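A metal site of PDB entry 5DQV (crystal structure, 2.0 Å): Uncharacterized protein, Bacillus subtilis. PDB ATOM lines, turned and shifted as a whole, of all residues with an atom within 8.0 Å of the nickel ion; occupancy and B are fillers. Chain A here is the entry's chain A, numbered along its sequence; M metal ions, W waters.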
ATOM      1  N   ASP A  32      15.455  32.033   7.431  1.00  0.00           N
ATOM      2  CA  ASP A  32      15.772  33.366   6.987  1.00  0.00           C
ATOM      3  C   ASP A  32      15.952  34.314   8.167  1.00  0.00           C
ATOM      4  O   ASP A  32      15.650  33.984   9.338  1.00  0.00           O
ATOM      5  CB  ASP A  32      14.754  33.915   5.980  1.00  0.00           C
ATOM      6  CG  ASP A  32      13.667  34.789   6.622  1.00  0.00           C
ATOM      7  OD1 ASP A  32      12.893  34.383   7.573  1.00  0.00           O
ATOM      8  OD2 ASP A  32      13.577  35.928   6.102  1.00  0.00           O
ATOM      9  N   HIS A  35      13.214  35.124  10.749  1.00  0.00           N
ATOM     10  CA  HIS A  35      12.961  33.988  11.636  1.00  0.00           C
ATOM     11  C   HIS A  35      14.036  33.954  12.709  1.00  0.00           C
ATOM     12  O   HIS A  35      13.746  33.893  13.898  1.00  0.00           O
ATOM     13  CB  HIS A  35      12.925  32.667  10.823  1.00  0.00           C
ATOM     14  CG  HIS A  35      13.008  31.449  11.683  1.00  0.00           C
ATOM     15  ND1 HIS A  35      12.010  31.085  12.551  1.00  0.00           N
ATOM     16  CD2 HIS A  35      14.006  30.551  11.877  1.00  0.00           C
ATOM     17  CE1 HIS A  35      12.361  29.987  13.191  1.00  0.00           C
ATOM     18  NE2 HIS A  35      13.577  29.650  12.799  1.00  0.00           N
ATOM     19  N   ILE A  36      15.310  34.014  12.295  1.00  0.00           N
ATOM     20  CA  ILE A  36      16.401  33.932  13.237  1.00  0.00           C
ATOM     21  C   ILE A  36      16.336  35.078  14.251  1.00  0.00           C
ATOM     22  O   ILE A  36      16.444  34.854  15.431  1.00  0.00           O
ATOM     23  CB  ILE A  36      17.757  33.893  12.499  1.00  0.00           C
ATOM     24  CG1 ILE A  36      17.910  32.506  11.871  1.00  0.00           C
ATOM     25  CG2 ILE A  36      18.861  34.234  13.483  1.00  0.00           C
ATOM     26  CD1 ILE A  36      19.001  32.506  10.819  1.00  0.00           C
ATOM     27  N   VAL A  39      13.580  34.336  16.747  1.00  0.00           N
ATOM     28  CA  VAL A  39      13.972  33.241  17.619  1.00  0.00           C
ATOM     29  C   VAL A  39      15.012  33.652  18.651  1.00  0.00           C
ATOM     30  O   VAL A  39      14.856  33.297  19.814  1.00  0.00           O
ATOM     31  CB  VAL A  39      14.387  32.006  16.843  1.00  0.00           C
ATOM     32  CG1 VAL A  39      15.017  30.951  17.793  1.00  0.00           C
ATOM     33  CG2 VAL A  39      13.251  31.506  16.057  1.00  0.00           C
ATOM     34  N   ALA A  61      20.976  30.457  19.240  1.00  0.00           N
ATOM     35  CA  ALA A  61      19.770  30.881  18.510  1.00  0.00           C
ATOM     36  C   ALA A  61      20.173  31.494  17.197  1.00  0.00           C
ATOM     37  O   ALA A  61      19.596  31.214  16.157  1.00  0.00           O
ATOM     38  CB  ALA A  61      18.957  31.872  19.353  1.00  0.00           C
ATOM     39  N   HIS A  64      21.495  28.722  14.780  1.00  0.00           N
ATOM     40  CA  HIS A  64      20.790  27.436  14.872  1.00  0.00           C
ATOM     41  C   HIS A  64      20.413  26.874  13.497  1.00  0.00           C
ATOM     42  O   HIS A  64      20.374  25.658  13.333  1.00  0.00           O
ATOM     43  CB  HIS A  64      19.564  27.527  15.848  1.00  0.00           C
ATOM     44  CG  HIS A  64      18.260  27.924  15.219  1.00  0.00           C
ATOM     45  ND1 HIS A  64      17.863  29.245  15.094  1.00  0.00           N
ATOM     46  CD2 HIS A  64      17.235  27.183  14.725  1.00  0.00           C
ATOM     47  CE1 HIS A  64      16.684  29.294  14.487  1.00  0.00           C
ATOM     48  NE2 HIS A  64      16.274  28.058  14.256  1.00  0.00           N
ATOM     49  N   ASP A  65      20.214  27.758  12.511  1.00  0.00           N
ATOM     50  CA  ASP A  65      19.732  27.352  11.187  1.00  0.00           C
ATOM     51  C   ASP A  65      20.839  27.191  10.136  1.00  0.00           C
ATOM     52  O   ASP A  65      20.525  26.775   8.989  1.00  0.00           O
ATOM     53  CB  ASP A  65      18.879  28.487  10.563  1.00  0.00           C
ATOM     54  CG  ASP A  65      17.401  28.318  10.754  1.00  0.00           C
ATOM     55  OD1 ASP A  65      16.915  27.456  11.556  1.00  0.00           O
ATOM     56  OD2 ASP A  65      16.699  29.134  10.080  1.00  0.00           O
ATOM     57  N   LEU A  66      22.068  27.609  10.436  1.00  0.00           N
ATOM     58  CA  LEU A  66      23.043  27.843   9.378  1.00  0.00           C
ATOM     59  C   LEU A  66      23.451  26.489   8.756  1.00  0.00           C
ATOM     60  O   LEU A  66      23.877  26.453   7.623  1.00  0.00           O
ATOM     61  CB  LEU A  66      24.290  28.562   9.885  1.00  0.00           C
ATOM     62  CG  LEU A  66      24.172  30.043  10.316  1.00  0.00           C
ATOM     63  CD1 LEU A  66      25.516  30.475  10.762  1.00  0.00           C
ATOM     64  CD2 LEU A  66      23.644  30.914   9.166  1.00  0.00           C
ATOM     65  N   ASP A  68      21.312  23.807   8.681  1.00  0.00           N
ATOM     66  CA  ASP A  68      20.080  23.023   8.564  1.00  0.00           C
ATOM     67  C   ASP A  68      19.933  22.628   7.089  1.00  0.00           C
ATOM     68  O   ASP A  68      20.211  23.412   6.159  1.00  0.00           O
ATOM     69  CB  ASP A  68      18.898  23.844   9.126  1.00  0.00           C
ATOM     70  CG  ASP A  68      17.549  23.063   9.151  1.00  0.00           C
ATOM     71  OD1 ASP A  68      16.981  22.816   8.100  1.00  0.00           O
ATOM     72  OD2 ASP A  68      17.057  22.767  10.242  1.00  0.00           O
ATOM     73  N   MET A 106      20.022  19.641  17.664  1.00  0.00           N
ATOM     74  CA  MET A 106      18.749  20.179  17.116  1.00  0.00           C
ATOM     75  C   MET A 106      18.528  19.700  15.677  1.00  0.00           C
ATOM     76  O   MET A 106      17.465  19.255  15.338  1.00  0.00           O
ATOM     77  CB  MET A 106      18.712  21.719  17.130  1.00  0.00           C
ATOM     78  CG  MET A 106      18.476  22.413  18.497  1.00  0.00           C
ATOM     79  SD  MET A 106      18.353  24.262  18.293  1.00  0.00           S
ATOM     80  CE  MET A 106      16.757  24.249  17.410  1.00  0.00           C
ATOM     81  N   VAL A 126      16.555  27.259  23.263  1.00  0.00           N
ATOM     82  CA  VAL A 126      16.578  27.558  21.820  1.00  0.00           C
ATOM     83  C   VAL A 126      15.511  26.784  21.074  1.00  0.00           C
ATOM     84  O   VAL A 126      14.813  27.327  20.183  1.00  0.00           O
ATOM     85  CB  VAL A 126      17.973  27.326  21.231  1.00  0.00           C
ATOM     86  CG1 VAL A 126      17.962  27.555  19.716  1.00  0.00           C
ATOM     87  CG2 VAL A 126      19.054  28.261  21.937  1.00  0.00           C
ATOM     88  N   GLN A 127      15.381  25.502  21.422  1.00  0.00           N
ATOM     89  CA  GLN A 127      14.424  24.621  20.766  1.00  0.00           C
ATOM     90  C   GLN A 127      13.021  25.169  20.968  1.00  0.00           C
ATOM     91  O   GLN A 127      12.242  25.272  20.029  1.00  0.00           O
ATOM     92  CB  GLN A 127      14.578  23.179  21.280  1.00  0.00           C
ATOM     93  CG  GLN A 127      13.608  22.198  20.677  1.00  0.00           C
ATOM     94  CD  GLN A 127      13.858  20.765  21.107  1.00  0.00           C
ATOM     95  OE1 GLN A 127      13.680  20.415  22.278  1.00  0.00           O
ATOM     96  NE2 GLN A 127      14.302  19.953  20.184  1.00  0.00           N
ATOM     97  N   ALA A 129      12.083  28.267  21.671  1.00  0.00           N
ATOM     98  CA  ALA A 129      11.926  29.516  20.956  1.00  0.00           C
ATOM     99  C   ALA A 129      11.648  29.244  19.459  1.00  0.00           C
ATOM    100  O   ALA A 129      10.785  29.868  18.832  1.00  0.00           O
ATOM    101  CB  ALA A 129      13.195  30.397  21.149  1.00  0.00           C
ATOM    102  N   ASP A 130      12.349  28.254  18.917  1.00  0.00           N
ATOM    103  CA  ASP A 130      12.224  27.906  17.522  1.00  0.00           C
ATOM    104  C   ASP A 130      10.813  27.379  17.274  1.00  0.00           C
ATOM    105  O   ASP A 130      10.152  27.696  16.237  1.00  0.00           O
ATOM    106  CB  ASP A 130      13.315  26.859  17.199  1.00  0.00           C
ATOM    107  CG  ASP A 130      13.561  26.684  15.759  1.00  0.00           C
ATOM    108  OD1 ASP A 130      13.411  27.605  14.993  1.00  0.00           O
ATOM    109  OD2 ASP A 130      13.931  25.581  15.360  1.00  0.00           O
ATOM    110  N   ARG A 131      10.331  26.539  18.206  1.00  0.00           N
ATOM    111  CA  ARG A 131       8.979  25.998  18.079  1.00  0.00           C
ATOM    112  C   ARG A 131       7.868  27.022  18.325  1.00  0.00           C
ATOM    113  O   ARG A 131       6.854  27.016  17.667  1.00  0.00           O
ATOM    114  CB  ARG A 131       8.799  24.713  18.943  1.00  0.00           C
ATOM    115  CG  ARG A 131       9.649  23.629  18.384  1.00  0.00           C
ATOM    116  CD  ARG A 131       9.470  22.367  19.114  1.00  0.00           C
ATOM    117  NE  ARG A 131      10.388  21.373  18.611  1.00  0.00           N
ATOM    118  CZ  ARG A 131      10.259  20.070  18.757  1.00  0.00           C
ATOM    119  NH1 ARG A 131       9.178  19.568  19.341  1.00  0.00           N
ATOM    120  NH2 ARG A 131      11.198  19.261  18.279  1.00  0.00           N
ATOM    121  N   ASP A 133       7.995  29.994  17.396  1.00  0.00           N
ATOM    122  CA  ASP A 133       7.892  30.791  16.177  1.00  0.00           C
ATOM    123  C   ASP A 133       7.070  30.053  15.089  1.00  0.00           C
ATOM    124  O   ASP A 133       6.711  30.635  14.090  1.00  0.00           O
ATOM    125  CB  ASP A 133       9.302  31.158  15.646  1.00  0.00           C
ATOM    126  CG  ASP A 133       9.284  32.235  14.592  1.00  0.00           C
ATOM    127  OD1 ASP A 133       8.859  33.353  14.900  1.00  0.00           O
ATOM    128  OD2 ASP A 133       9.740  31.988  13.433  1.00  0.00           O
ATOM    129  N   ARG A 142       3.569  31.593   8.714  1.00  0.00           N
ATOM    130  CA  ARG A 142       4.676  30.811   8.189  1.00  0.00           C
ATOM    131  C   ARG A 142       4.173  29.565   7.465  1.00  0.00           C
ATOM    132  O   ARG A 142       4.714  29.199   6.421  1.00  0.00           O
ATOM    133  CB  ARG A 142       5.669  30.473   9.285  1.00  0.00           C
ATOM    134  CG  ARG A 142       6.473  31.650   9.757  1.00  0.00           C
ATOM    135  CD  ARG A 142       7.409  31.240  10.874  1.00  0.00           C
ATOM    136  NE  ARG A 142       8.489  30.436  10.315  1.00  0.00           N
ATOM    137  CZ  ARG A 142       9.171  29.482  10.938  1.00  0.00           C
ATOM    138  NH1 ARG A 142       8.943  29.146  12.208  1.00  0.00           N
ATOM    139  NH2 ARG A 142      10.123  28.859  10.263  1.00  0.00           N
HETATM  140 NI    NI M   1      14.625  27.788  13.171  1.00  0.00          NI
HETATM  141  O   HOH W   1      12.490  26.891  11.885  1.00  0.00           O
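N of His 35 lies within hydrogen-bond range of OD1 of Asp 32 (3.3 Å). OD1 of Asp 65 lies close to NE2 of His 64, 2.8 Å away. ND1 of His 64 is in hydrogen-bond range of O of Ala 61. OD2 of Asp 133 sits at hydrogen-bond distance from ND1 of His 35.
Within 4 Å of the nickel ion: His 35, His 64, Asp 65 and Asp 130.
The nickel ion is bound by NE2 of His 64 (2.0 Å), NE2 of His 35 (2.2 Å) and OD1 of Asp 130 (2.2 Å). The nickel ion has three donor atoms within binding distance. Slightly farther from the nickel ion lies water W1 (2.6 Å). Slightly farther from the nickel ion lies the side-chain carboxylate (OD1) of Asp 65 (2.8 Å).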
